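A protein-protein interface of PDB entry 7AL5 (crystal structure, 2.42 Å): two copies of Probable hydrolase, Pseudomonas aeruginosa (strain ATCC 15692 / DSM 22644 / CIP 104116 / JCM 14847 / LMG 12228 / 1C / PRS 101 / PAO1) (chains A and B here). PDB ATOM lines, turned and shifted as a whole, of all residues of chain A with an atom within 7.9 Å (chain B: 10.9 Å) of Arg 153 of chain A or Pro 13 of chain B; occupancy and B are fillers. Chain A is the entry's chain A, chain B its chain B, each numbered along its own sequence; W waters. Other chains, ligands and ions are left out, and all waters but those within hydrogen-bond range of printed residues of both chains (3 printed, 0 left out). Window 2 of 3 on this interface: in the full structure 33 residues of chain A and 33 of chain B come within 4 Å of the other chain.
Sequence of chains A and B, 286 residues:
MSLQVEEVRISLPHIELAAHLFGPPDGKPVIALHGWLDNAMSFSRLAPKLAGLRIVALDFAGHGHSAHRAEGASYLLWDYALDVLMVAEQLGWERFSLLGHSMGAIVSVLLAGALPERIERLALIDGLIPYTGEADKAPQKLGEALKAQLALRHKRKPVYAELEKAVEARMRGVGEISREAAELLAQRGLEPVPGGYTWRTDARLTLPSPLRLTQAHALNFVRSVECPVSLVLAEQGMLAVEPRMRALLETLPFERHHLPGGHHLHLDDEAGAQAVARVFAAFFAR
The backbone carbonyl oxygen (O) of Arg 153 of chain A lies within hydrogen-bond range of the guanidinium group (NH1) of Arg 156 of chain A (3.0 Å).
The side-chain carboxylate (OD1) of Asp 83 of chain B is in hydrogen-bond range of a ring nitrogen (NE2) of His 14 of chain B, 3.0 Å away.
Ala 70 of chain B touches Glu 71 of chain A (CB to O, 3.5 Å).
Gly 72 of chain A touches His 14 of chain B (N to CB, 3.7 Å).
CD of Gln 149 of chain A touches CD2 of Leu 82 of chain B, 3.7 Å away.
CD2 of Leu 85 of chain B touches CD1 of Leu 150 of chain A, at 3.8 Å.
Met 86 of chain B touches Leu 150 of chain A (CG to CD2, 3.8 Å).
Leu 150 of chain A touches Glu 89 of chain B (CD2 to CG, 3.9 Å).
Arg 153 of chain A touches Pro 13 of chain B (NH1 to CG, 3.9 Å).
Arg 153 of chain A touches one residue of chain B.
Pro 13 of chain B touches just one residue of chain A: Arg 153.
No residue of chain B comes within 4 Å of Leu 152 of chain A.
No residue of chain B comes within 4 Å of His 154 of chain A.
Of the printed residues of chain A, His 14 of chain B touches Gly 72.
Of the printed residues of chain B, Glu 71 of chain A touches Ala 70 (3.5 Å).
Of the printed residues of chain B, Gln 149 of chain A touches Leu 82 (3.7 Å).
Leu 91 of chain B touches none of the printed residues of chain A.
Ile 15 of chain B touches none of the printed residues of chain A.
The nearest residue of chain B that does not touch Arg 153 of chain A is Met 86 of chain B (4.2 Å).
The nearest residue of chain A that does not touch Pro 13 of chain B is Glu 71 of chain A (4.3 Å).
The nearest printed residue of chain A that does not touch Met 86 of chain B is Gln 149 of chain A (4.1 Å).
Of the 24 printed residues of chain B, 7 touch a printed residue of chain A.
Hydrophobic or aromatic side chains of chain B within 4 Å of the printed part of chain A: Pro 13, His 14, Ala 70, Leu 82, Leu 85 and Met 86.
Among the printed residues, no Asp or Glu carboxylate lies within 4 Å of a Lys or Arg side-chain nitrogen of the other chain.
No position is printed for both chains.
Of the 7 pairs that touch across the chains among the printed residues, none has its exchanged pair printed and touching as well.
Water W1 lies within hydrogen-bond range of the guanidinium group (NH1) of Arg 153 of chain A (2.8 Å) and the side-chain amide oxygen (OE1) of Gln 90 of chain B (2.9 Å).
Water W2 lies within hydrogen-bond range of the backbone carbonyl oxygen of Glu 71 of chain A (2.8 Å), the backbone NH of Ala 70 of chain B (2.9 Å) and the backbone carbonyl oxygen of His 14 of chain B (3.0 Å).
Water W3 bridges O of Gly 72 of chain A (3.0 Å) and NH1 of Arg 69 of chain B (3.2 Å).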
ATOM      1  N   GLU A  71      29.140   6.573 -17.715  1.00  0.00           N
ATOM      2  CA  GLU A  71      28.467   6.644 -16.403  1.00  0.00           C
ATOM      3  C   GLU A  71      29.501   6.726 -15.286  1.00  0.00           C
ATOM      4  O   GLU A  71      30.381   5.939 -15.291  1.00  0.00           O
ATOM      5  CB  GLU A  71      27.581   5.411 -16.271  1.00  0.00           C
ATOM      6  CG  GLU A  71      26.126   5.746 -16.121  1.00  0.00           C
ATOM      7  CD  GLU A  71      25.300   5.637 -17.383  1.00  0.00           C
ATOM      8  OE1 GLU A  71      24.184   6.171 -17.414  1.00  0.00           O
ATOM      9  OE2 GLU A  71      25.760   4.995 -18.326  1.00  0.00           O
ATOM     10  N   GLY A  72      29.411   7.718 -14.416  1.00  0.00           N
ATOM     11  CA  GLY A  72      30.298   7.848 -13.255  1.00  0.00           C
ATOM     12  C   GLY A  72      31.595   8.615 -13.486  1.00  0.00           C
ATOM     13  O   GLY A  72      32.292   8.944 -12.514  1.00  0.00           O
ATOM     14  N   ALA A 148      25.499  17.442  -4.092  1.00  0.00           N
ATOM     15  CA  ALA A 148      25.098  17.736  -5.463  1.00  0.00           C
ATOM     16  C   ALA A 148      25.074  16.469  -6.308  1.00  0.00           C
ATOM     17  O   ALA A 148      24.193  16.309  -7.166  1.00  0.00           O
ATOM     18  CB  ALA A 148      26.015  18.784  -6.093  1.00  0.00           C
ATOM     19  N   GLN A 149      26.019  15.550  -6.068  1.00  0.00           N
ATOM     20  CA  GLN A 149      26.013  14.302  -6.817  1.00  0.00           C
ATOM     21  C   GLN A 149      24.745  13.512  -6.538  1.00  0.00           C
ATOM     22  O   GLN A 149      24.233  12.824  -7.418  1.00  0.00           O
ATOM     23  CB  GLN A 149      27.231  13.447  -6.473  1.00  0.00           C
ATOM     24  CG  GLN A 149      28.525  13.953  -7.074  1.00  0.00           C
ATOM     25  CD  GLN A 149      28.854  13.316  -8.420  1.00  0.00           C
ATOM     26  OE1 GLN A 149      27.971  12.827  -9.131  1.00  0.00           O
ATOM     27  NE2 GLN A 149      30.134  13.365  -8.793  1.00  0.00           N
ATOM     28  N   LEU A 150      24.256  13.573  -5.301  1.00  0.00           N
ATOM     29  CA  LEU A 150      23.060  12.844  -4.919  1.00  0.00           C
ATOM     30  C   LEU A 150      21.822  13.451  -5.562  1.00  0.00           C
ATOM     31  O   LEU A 150      20.876  12.738  -5.898  1.00  0.00           O
ATOM     32  CB  LEU A 150      22.937  12.868  -3.391  1.00  0.00           C
ATOM     33  CG  LEU A 150      23.806  11.942  -2.540  1.00  0.00           C
ATOM     34  CD1 LEU A 150      23.395  12.106  -1.086  1.00  0.00           C
ATOM     35  CD2 LEU A 150      23.701  10.473  -2.929  1.00  0.00           C
ATOM     36  N   ALA A 151      21.828  14.751  -5.746  1.00  0.00           N
ATOM     37  CA  ALA A 151      20.727  15.526  -6.297  1.00  0.00           C
ATOM     38  C   ALA A 151      20.779  15.636  -7.815  1.00  0.00           C
ATOM     39  O   ALA A 151      19.917  16.288  -8.410  1.00  0.00           O
ATOM     40  CB  ALA A 151      20.767  16.926  -5.669  1.00  0.00           C
ATOM     41  N   LEU A 152      21.759  14.998  -8.447  1.00  0.00           N
ATOM     42  CA  LEU A 152      21.984  15.158  -9.878  1.00  0.00           C
ATOM     43  C   LEU A 152      20.901  14.514 -10.733  1.00  0.00           C
ATOM     44  O   LEU A 152      20.676  14.958 -11.862  1.00  0.00           O
ATOM     45  CB  LEU A 152      23.324  14.552 -10.243  1.00  0.00           C
ATOM     46  CG  LEU A 152      23.773  14.684 -11.695  1.00  0.00           C
ATOM     47  CD1 LEU A 152      24.508  16.006 -11.898  1.00  0.00           C
ATOM     48  CD2 LEU A 152      24.621  13.483 -12.060  1.00  0.00           C
ATOM     49  N   ARG A 153      20.266  13.438 -10.255  1.00  0.00           N
ATOM     50  CA  ARG A 153      19.239  12.766 -11.047  1.00  0.00           C
ATOM     51  C   ARG A 153      18.121  13.721 -11.452  1.00  0.00           C
ATOM     52  O   ARG A 153      17.405  13.451 -12.417  1.00  0.00           O
ATOM     53  CB  ARG A 153      18.657  11.573 -10.255  1.00  0.00           C
ATOM     54  CG  ARG A 153      18.446  11.925  -8.774  1.00  0.00           C
ATOM     55  CD  ARG A 153      17.638  10.970  -7.893  1.00  0.00           C
ATOM     56  NE  ARG A 153      17.790   9.530  -8.087  1.00  0.00           N
ATOM     57  CZ  ARG A 153      18.786   8.786  -7.606  1.00  0.00           C
ATOM     58  NH1 ARG A 153      18.770   7.467  -7.815  1.00  0.00           N
ATOM     59  NH2 ARG A 153      19.802   9.350  -6.946  1.00  0.00           N
ATOM     60  N   HIS A 154      17.957  14.828 -10.735  1.00  0.00           N
ATOM     61  CA  HIS A 154      16.819  15.713 -10.900  1.00  0.00           C
ATOM     62  C   HIS A 154      17.097  16.891 -11.828  1.00  0.00           C
ATOM     63  O   HIS A 154      16.180  17.675 -12.113  1.00  0.00           O
ATOM     64  CB  HIS A 154      16.371  16.213  -9.516  1.00  0.00           C
ATOM     65  CG  HIS A 154      15.898  15.112  -8.598  1.00  0.00           C
ATOM     66  ND1 HIS A 154      16.236  15.051  -7.260  1.00  0.00           N
ATOM     67  CD2 HIS A 154      15.109  14.035  -8.832  1.00  0.00           C
ATOM     68  CE1 HIS A 154      15.675  13.985  -6.712  1.00  0.00           C
ATOM     69  NE2 HIS A 154      15.003  13.342  -7.647  1.00  0.00           N
ATOM     70  N   LYS A 155      18.330  17.030 -12.314  1.00  0.00           N
ATOM     71  CA  LYS A 155      18.660  18.065 -13.284  1.00  0.00           C
ATOM     72  C   LYS A 155      17.960  17.815 -14.633  1.00  0.00           C
ATOM     73  O   LYS A 155      17.853  16.683 -15.120  1.00  0.00           O
ATOM     74  CB  LYS A 155      20.184  18.113 -13.475  1.00  0.00           C
ATOM     75  CG  LYS A 155      21.004  18.703 -12.319  1.00  0.00           C
ATOM     76  CD  LYS A 155      20.640  20.156 -11.989  1.00  0.00           C
ATOM     77  CE  LYS A 155      21.458  20.677 -10.797  1.00  0.00           C
ATOM     78  NZ  LYS A 155      21.128  22.098 -10.438  1.00  0.00           N
ATOM     79  N   ARG A 156      17.469  18.885 -15.245  1.00  0.00           N
ATOM     80  CA  ARG A 156      16.889  18.791 -16.576  1.00  0.00           C
ATOM     81  C   ARG A 156      17.424  19.956 -17.367  1.00  0.00           C
ATOM     82  O   ARG A 156      17.922  20.918 -16.791  1.00  0.00           O
ATOM     83  CB  ARG A 156      15.359  18.835 -16.584  1.00  0.00           C
ATOM     84  CG  ARG A 156      14.692  17.703 -15.847  1.00  0.00           C
ATOM     85  CD  ARG A 156      14.725  16.404 -16.613  1.00  0.00           C
ATOM     86  NE  ARG A 156      14.113  15.340 -15.812  1.00  0.00           N
ATOM     87  CZ  ARG A 156      14.770  14.591 -14.920  1.00  0.00           C
ATOM     88  NH1 ARG A 156      16.073  14.777 -14.715  1.00  0.00           N
ATOM     89  NH2 ARG A 156      14.129  13.651 -14.228  1.00  0.00           N
ATOM     90  N   ALA A 203      24.563  16.836 -17.632  1.00  0.00           N
ATOM     91  CA  ALA A 203      24.186  17.443 -16.355  1.00  0.00           C
ATOM     92  C   ALA A 203      25.361  17.491 -15.374  1.00  0.00           C
ATOM     93  O   ALA A 203      25.406  18.366 -14.508  1.00  0.00           O
ATOM     94  CB  ALA A 203      23.034  16.678 -15.724  1.00  0.00           C
ATOM     95  N   LEU A 207      28.167  20.061 -11.690  1.00  0.00           N
ATOM     96  CA  LEU A 207      28.579  19.683 -10.343  1.00  0.00           C
ATOM     97  C   LEU A 207      29.744  20.541  -9.859  1.00  0.00           C
ATOM     98  O   LEU A 207      30.598  20.932 -10.646  1.00  0.00           O
ATOM     99  CB  LEU A 207      29.004  18.219 -10.300  1.00  0.00           C
ATOM    100  CG  LEU A 207      27.958  17.123 -10.507  1.00  0.00           C
ATOM    101  CD1 LEU A 207      28.693  15.811 -10.837  1.00  0.00           C
ATOM    102  CD2 LEU A 207      27.024  16.951  -9.300  1.00  0.00           C
ATOM    103  N   ARG B   9      23.802  -7.718  -4.416  1.00  0.00           N
ATOM    104  CA  ARG B   9      24.239  -6.690  -5.371  1.00  0.00           C
ATOM    105  C   ARG B   9      23.528  -5.409  -4.963  1.00  0.00           C
ATOM    106  O   ARG B   9      22.362  -5.441  -4.679  1.00  0.00           O
ATOM    107  CB  ARG B   9      23.855  -6.978  -6.819  1.00  0.00           C
ATOM    108  CG  ARG B   9      24.218  -8.350  -7.346  1.00  0.00           C
ATOM    109  CD  ARG B   9      25.694  -8.553  -7.474  1.00  0.00           C
ATOM    110  NE  ARG B   9      26.307  -7.612  -8.373  1.00  0.00           N
ATOM    111  CZ  ARG B   9      27.588  -7.572  -8.629  1.00  0.00           C
ATOM    112  NH1 ARG B   9      28.395  -8.429  -8.048  1.00  0.00           N
ATOM    113  NH2 ARG B   9      28.067  -6.674  -9.456  1.00  0.00           N
ATOM    114  N   ILE B  10      24.243  -4.317  -4.876  1.00  0.00           N
ATOM    115  CA  ILE B  10      23.666  -3.010  -4.600  1.00  0.00           C
ATOM    116  C   ILE B  10      23.789  -2.173  -5.870  1.00  0.00           C
ATOM    117  O   ILE B  10      24.881  -2.015  -6.429  1.00  0.00           O
ATOM    118  CB  ILE B  10      24.342  -2.350  -3.391  1.00  0.00           C
ATOM    119  CG1 ILE B  10      24.210  -3.269  -2.175  1.00  0.00           C
ATOM    120  CG2 ILE B  10      23.680  -1.040  -3.065  1.00  0.00           C
ATOM    121  CD1 ILE B  10      25.082  -2.904  -0.997  1.00  0.00           C
ATOM    122  N   SER B  11      22.662  -1.681  -6.340  1.00  0.00           N
ATOM    123  CA  SER B  11      22.577  -0.928  -7.603  1.00  0.00           C
ATOM    124  C   SER B  11      22.670   0.571  -7.352  1.00  0.00           C
ATOM    125  O   SER B  11      21.779   1.098  -6.774  1.00  0.00           O
ATOM    126  CB  SER B  11      21.329  -1.270  -8.315  1.00  0.00           C
ATOM    127  OG  SER B  11      21.353  -2.610  -8.680  1.00  0.00           O
ATOM    128  N   LEU B  12      23.753   1.214  -7.748  1.00  0.00           N
ATOM    129  CA  LEU B  12      23.869   2.680  -7.696  1.00  0.00           C
ATOM    130  C   LEU B  12      23.575   3.211  -9.106  1.00  0.00           C
ATOM    131  O   LEU B  12      23.602   2.454 -10.035  1.00  0.00           O
ATOM    132  CB  LEU B  12      25.247   3.075  -7.174  1.00  0.00           C
ATOM    133  CG  LEU B  12      25.755   2.268  -5.985  1.00  0.00           C
ATOM    134  CD1 LEU B  12      27.096   2.778  -5.519  1.00  0.00           C
ATOM    135  CD2 LEU B  12      24.775   2.286  -4.842  1.00  0.00           C
ATOM    136  N   PRO B  13      23.281   4.495  -9.339  1.00  0.00           N
ATOM    137  CA  PRO B  13      22.973   4.930 -10.690  1.00  0.00           C
ATOM    138  C   PRO B  13      24.086   4.679 -11.716  1.00  0.00           C
ATOM    139  O   PRO B  13      23.797   4.330 -12.795  1.00  0.00           O
ATOM    140  CB  PRO B  13      22.737   6.430 -10.541  1.00  0.00           C
ATOM    141  CG  PRO B  13      22.363   6.614  -9.106  1.00  0.00           C
ATOM    142  CD  PRO B  13      23.144   5.569  -8.363  1.00  0.00           C
ATOM    143  N   HIS B  14      25.332   4.795 -11.307  1.00  0.00           N
ATOM    144  CA  HIS B  14      26.489   4.727 -12.180  1.00  0.00           C
ATOM    145  C   HIS B  14      27.292   3.432 -12.090  1.00  0.00           C
ATOM    146  O   HIS B  14      28.239   3.289 -12.874  1.00  0.00           O
ATOM    147  CB  HIS B  14      27.440   5.884 -11.850  1.00  0.00           C
ATOM    148  CG  HIS B  14      27.898   5.895 -10.424  1.00  0.00           C
ATOM    149  ND1 HIS B  14      27.051   6.160  -9.367  1.00  0.00           N
ATOM    150  CD2 HIS B  14      29.113   5.667  -9.877  1.00  0.00           C
ATOM    151  CE1 HIS B  14      27.725   6.090  -8.234  1.00  0.00           C
ATOM    152  NE2 HIS B  14      28.986   5.821  -8.518  1.00  0.00           N
ATOM    153  N   ILE B  15      27.003   2.535 -11.160  1.00  0.00           N
ATOM    154  CA  ILE B  15      27.828   1.335 -10.966  1.00  0.00           C
ATOM    155  C   ILE B  15      27.088   0.350 -10.089  1.00  0.00           C
ATOM    156  O   ILE B  15      26.263   0.741  -9.261  1.00  0.00           O
ATOM    157  CB  ILE B  15      29.200   1.705 -10.336  1.00  0.00           C
ATOM    158  CG1 ILE B  15      30.119   0.478 -10.346  1.00  0.00           C
ATOM    159  CG2 ILE B  15      28.999   2.208  -8.914  1.00  0.00           C
ATOM    160  CD1 ILE B  15      31.574   0.807 -10.242  1.00  0.00           C
ATOM    161  N   GLU B  16      27.471  -0.915 -10.175  1.00  0.00           N
ATOM    162  CA  GLU B  16      26.827  -1.958  -9.387  1.00  0.00           C
ATOM    163  C   GLU B  16      27.852  -2.649  -8.499  1.00  0.00           C
ATOM    164  O   GLU B  16      28.824  -3.218  -8.994  1.00  0.00           O
ATOM    165  CB  GLU B  16      26.131  -2.959 -10.307  1.00  0.00           C
ATOM    166  CG  GLU B  16      25.234  -3.894  -9.608  1.00  0.00           C
ATOM    167  CD  GLU B  16      24.696  -4.998 -10.522  1.00  0.00           C
ATOM    168  OE1 GLU B  16      23.776  -4.722 -11.343  1.00  0.00           O
ATOM    169  OE2 GLU B  16      25.179  -6.148 -10.367  1.00  0.00           O
ATOM    170  N   LEU B  17      27.632  -2.604  -7.195  1.00  0.00           N
ATOM    171  CA  LEU B  17      28.576  -3.149  -6.229  1.00  0.00           C
ATOM    172  C   LEU B  17      28.070  -4.472  -5.670  1.00  0.00           C
ATOM    173  O   LEU B  17      26.893  -4.806  -5.780  1.00  0.00           O
ATOM    174  CB  LEU B  17      28.807  -2.152  -5.086  1.00  0.00           C
ATOM    175  CG  LEU B  17      29.283  -0.758  -5.528  1.00  0.00           C
ATOM    176  CD1 LEU B  17      29.415   0.215  -4.328  1.00  0.00           C
ATOM    177  CD2 LEU B  17      30.622  -0.818  -6.365  1.00  0.00           C
ATOM    178  N   ALA B  67      31.495  -4.404  -9.615  1.00  0.00           N
ATOM    179  CA  ALA B  67      31.846  -4.135 -10.999  1.00  0.00           C
ATOM    180  C   ALA B  67      33.034  -3.187 -11.071  1.00  0.00           C
ATOM    181  O   ALA B  67      33.317  -2.432 -10.133  1.00  0.00           O
ATOM    182  CB  ALA B  67      30.666  -3.548 -11.758  1.00  0.00           C
ATOM    183  N   HIS B  68      33.759  -3.272 -12.189  1.00  0.00           N
ATOM    184  CA  HIS B  68      34.752  -2.269 -12.529  1.00  0.00           C
ATOM    185  C   HIS B  68      34.034  -0.996 -12.956  1.00  0.00           C
ATOM    186  O   HIS B  68      32.890  -1.029 -13.430  1.00  0.00           O
ATOM    187  CB  HIS B  68      35.667  -2.740 -13.656  1.00  0.00           C
ATOM    188  CG  HIS B  68      36.405  -4.004 -13.359  1.00  0.00           C
ATOM    189  ND1 HIS B  68      37.260  -4.142 -12.289  1.00  0.00           N
ATOM    190  CD2 HIS B  68      36.412  -5.197 -14.000  1.00  0.00           C
ATOM    191  CE1 HIS B  68      37.762  -5.361 -12.278  1.00  0.00           C
ATOM    192  NE2 HIS B  68      37.262  -6.024 -13.306  1.00  0.00           N
ATOM    193  N   ARG B  69      34.693   0.135 -12.759  1.00  0.00           N
ATOM    194  CA  ARG B  69      34.072   1.373 -13.186  1.00  0.00           C
ATOM    195  C   ARG B  69      33.976   1.394 -14.706  1.00  0.00           C
ATOM    196  O   ARG B  69      34.657   0.650 -15.401  1.00  0.00           O
ATOM    197  CB  ARG B  69      34.869   2.570 -12.689  1.00  0.00           C
ATOM    198  CG  ARG B  69      34.945   2.701 -11.182  1.00  0.00           C
ATOM    199  CD  ARG B  69      35.249   4.174 -10.811  1.00  0.00           C
ATOM    200  NE  ARG B  69      35.484   4.304  -9.380  1.00  0.00           N
ATOM    201  CZ  ARG B  69      34.525   4.231  -8.453  1.00  0.00           C
ATOM    202  NH1 ARG B  69      33.225   4.093  -8.796  1.00  0.00           N
ATOM    203  NH2 ARG B  69      34.868   4.308  -7.164  1.00  0.00           N
ATOM    204  N   ALA B  70      33.144   2.291 -15.217  1.00  0.00           N
ATOM    205  CA  ALA B  70      33.023   2.443 -16.649  1.00  0.00           C
ATOM    206  C   ALA B  70      34.293   3.042 -17.218  1.00  0.00           C
ATOM    207  O   ALA B  70      35.103   3.603 -16.504  1.00  0.00           O
ATOM    208  CB  ALA B  70      31.821   3.319 -17.017  1.00  0.00           C
ATOM    209  N   ASP B  79      35.777   9.289  -5.070  1.00  0.00           N
ATOM    210  CA  ASP B  79      34.828   8.463  -5.809  1.00  0.00           C
ATOM    211  C   ASP B  79      34.361   7.290  -4.945  1.00  0.00           C
ATOM    212  O   ASP B  79      33.165   6.988  -4.928  1.00  0.00           O
ATOM    213  CB  ASP B  79      35.435   7.981  -7.137  1.00  0.00           C
ATOM    214  CG  ASP B  79      36.154   9.100  -7.908  1.00  0.00           C
ATOM    215  OD1 ASP B  79      35.578  10.215  -8.081  1.00  0.00           O
ATOM    216  OD2 ASP B  79      37.324   8.855  -8.325  1.00  0.00           O
ATOM    217  N   LEU B  82      31.846   8.872  -2.530  1.00  0.00           N
ATOM    218  CA  LEU B  82      30.534   9.028  -3.138  1.00  0.00           C
ATOM    219  C   LEU B  82      29.809   7.686  -3.220  1.00  0.00           C
ATOM    220  O   LEU B  82      28.608   7.607  -2.946  1.00  0.00           O
ATOM    221  CB  LEU B  82      30.646   9.646  -4.525  1.00  0.00           C
ATOM    222  CG  LEU B  82      29.258   9.674  -5.184  1.00  0.00           C
ATOM    223  CD1 LEU B  82      28.323  10.573  -4.351  1.00  0.00           C
ATOM    224  CD2 LEU B  82      29.326  10.144  -6.619  1.00  0.00           C
ATOM    225  N   ASP B  83      30.523   6.617  -3.562  1.00  0.00           N
ATOM    226  CA  ASP B  83      29.858   5.326  -3.683  1.00  0.00           C
ATOM    227  C   ASP B  83      29.265   4.890  -2.348  1.00  0.00           C
ATOM    228  O   ASP B  83      28.106   4.451  -2.276  1.00  0.00           O
ATOM    229  CB  ASP B  83      30.831   4.268  -4.192  1.00  0.00           C
ATOM    230  CG  ASP B  83      31.310   4.510  -5.630  1.00  0.00           C
ATOM    231  OD1 ASP B  83      30.948   5.522  -6.301  1.00  0.00           O
ATOM    232  OD2 ASP B  83      32.090   3.646  -6.078  1.00  0.00           O
ATOM    233  N   VAL B  84      30.028   5.041  -1.276  1.00  0.00           N
ATOM    234  CA  VAL B  84      29.626   4.600   0.079  1.00  0.00           C
ATOM    235  C   VAL B  84      28.320   5.308   0.430  1.00  0.00           C
ATOM    236  O   VAL B  84      27.400   4.644   0.869  1.00  0.00           O
ATOM    237  CB  VAL B  84      30.708   4.900   1.132  1.00  0.00           C
ATOM    238  CG1 VAL B  84      30.246   4.532   2.527  1.00  0.00           C
ATOM    239  CG2 VAL B  84      32.026   4.229   0.831  1.00  0.00           C
ATOM    240  N   LEU B  85      28.243   6.597   0.133  1.00  0.00           N
ATOM    241  CA  LEU B  85      27.076   7.457   0.398  1.00  0.00           C
ATOM    242  C   LEU B  85      25.850   6.969  -0.374  1.00  0.00           C
ATOM    243  O   LEU B  85      24.804   6.859   0.211  1.00  0.00           O
ATOM    244  CB  LEU B  85      27.446   8.877  -0.012  1.00  0.00           C
ATOM    245  CG  LEU B  85      26.463   9.946   0.422  1.00  0.00           C
ATOM    246  CD1 LEU B  85      26.250   9.908   1.921  1.00  0.00           C
ATOM    247  CD2 LEU B  85      26.941  11.302  -0.019  1.00  0.00           C
ATOM    248  N   MET B  86      26.017   6.667  -1.647  1.00  0.00           N
ATOM    249  CA  MET B  86      24.958   6.174  -2.545  1.00  0.00           C
ATOM    250  C   MET B  86      24.529   4.782  -2.069  1.00  0.00           C
ATOM    251  O   MET B  86      23.364   4.482  -2.165  1.00  0.00           O
ATOM    252  CB  MET B  86      25.449   6.293  -3.981  1.00  0.00           C
ATOM    253  CG  MET B  86      25.796   7.700  -4.341  1.00  0.00           C
ATOM    254  SD  MET B  86      25.714   8.081  -6.219  1.00  0.00           S
ATOM    255  CE  MET B  86      23.991   8.781  -6.562  1.00  0.00           C
ATOM    256  N   VAL B  87      25.446   3.943  -1.610  1.00  0.00           N
ATOM    257  CA  VAL B  87      25.021   2.684  -1.014  1.00  0.00           C
ATOM    258  C   VAL B  87      24.126   2.925   0.193  1.00  0.00           C
ATOM    259  O   VAL B  87      23.131   2.219   0.391  1.00  0.00           O
ATOM    260  CB  VAL B  87      26.232   1.812  -0.646  1.00  0.00           C
ATOM    261  CG1 VAL B  87      25.800   0.706   0.271  1.00  0.00           C
ATOM    262  CG2 VAL B  87      26.748   1.177  -1.923  1.00  0.00           C
ATOM    263  N   ALA B  88      24.488   3.885   1.052  1.00  0.00           N
ATOM    264  CA  ALA B  88      23.647   4.188   2.207  1.00  0.00           C
ATOM    265  C   ALA B  88      22.263   4.633   1.756  1.00  0.00           C
ATOM    266  O   ALA B  88      21.256   4.254   2.355  1.00  0.00           O
ATOM    267  CB  ALA B  88      24.308   5.264   3.059  1.00  0.00           C
ATOM    268  N   GLU B  89      22.201   5.413   0.677  1.00  0.00           N
ATOM    269  CA  GLU B  89      20.922   5.848   0.126  1.00  0.00           C
ATOM    270  C   GLU B  89      20.132   4.677  -0.425  1.00  0.00           C
ATOM    271  O   GLU B  89      18.915   4.599  -0.251  1.00  0.00           O
ATOM    272  CB  GLU B  89      21.151   6.883  -0.975  1.00  0.00           C
ATOM    273  CG  GLU B  89      21.735   8.207  -0.491  1.00  0.00           C
ATOM    274  CD  GLU B  89      20.691   9.090   0.163  1.00  0.00           C
ATOM    275  OE1 GLU B  89      19.859   9.645  -0.593  1.00  0.00           O
ATOM    276  OE2 GLU B  89      20.712   9.220   1.417  1.00  0.00           O
ATOM    277  N   GLN B  90      20.808   3.776  -1.117  1.00  0.00           N
ATOM    278  CA  GLN B  90      20.147   2.607  -1.675  1.00  0.00           C
ATOM    279  C   GLN B  90      19.598   1.706  -0.586  1.00  0.00           C
ATOM    280  O   GLN B  90      18.615   0.994  -0.803  1.00  0.00           O
ATOM    281  CB  GLN B  90      21.140   1.831  -2.544  1.00  0.00           C
ATOM    282  CG  GLN B  90      20.518   0.993  -3.600  1.00  0.00           C
ATOM    283  CD  GLN B  90      19.521   1.762  -4.465  1.00  0.00           C
ATOM    284  OE1 GLN B  90      19.687   2.951  -4.785  1.00  0.00           O
ATOM    285  NE2 GLN B  90      18.494   1.079  -4.846  1.00  0.00           N
ATOM    286  N   LEU B  91      20.228   1.694   0.577  1.00  0.00           N
ATOM    287  CA  LEU B  91      19.740   0.880   1.673  1.00  0.00           C
ATOM    288  C   LEU B  91      18.673   1.591   2.483  1.00  0.00           C
ATOM    289  O   LEU B  91      18.107   0.982   3.390  1.00  0.00           O
ATOM    290  CB  LEU B  91      20.894   0.484   2.598  1.00  0.00           C
ATOM    291  CG  LEU B  91      22.087  -0.315   2.057  1.00  0.00           C
ATOM    292  CD1 LEU B  91      23.150  -0.577   3.129  1.00  0.00           C
ATOM    293  CD2 LEU B  91      21.655  -1.639   1.497  1.00  0.00           C
HETATM  294  O   HOH W   1      19.924   5.484  -6.221  1.00  0.00           O
HETATM  295  O   HOH W   2      31.125   3.704 -13.703  1.00  0.00           O
HETATM  296  O   HOH W   3      32.470   6.810 -10.374  1.00  0.00           O
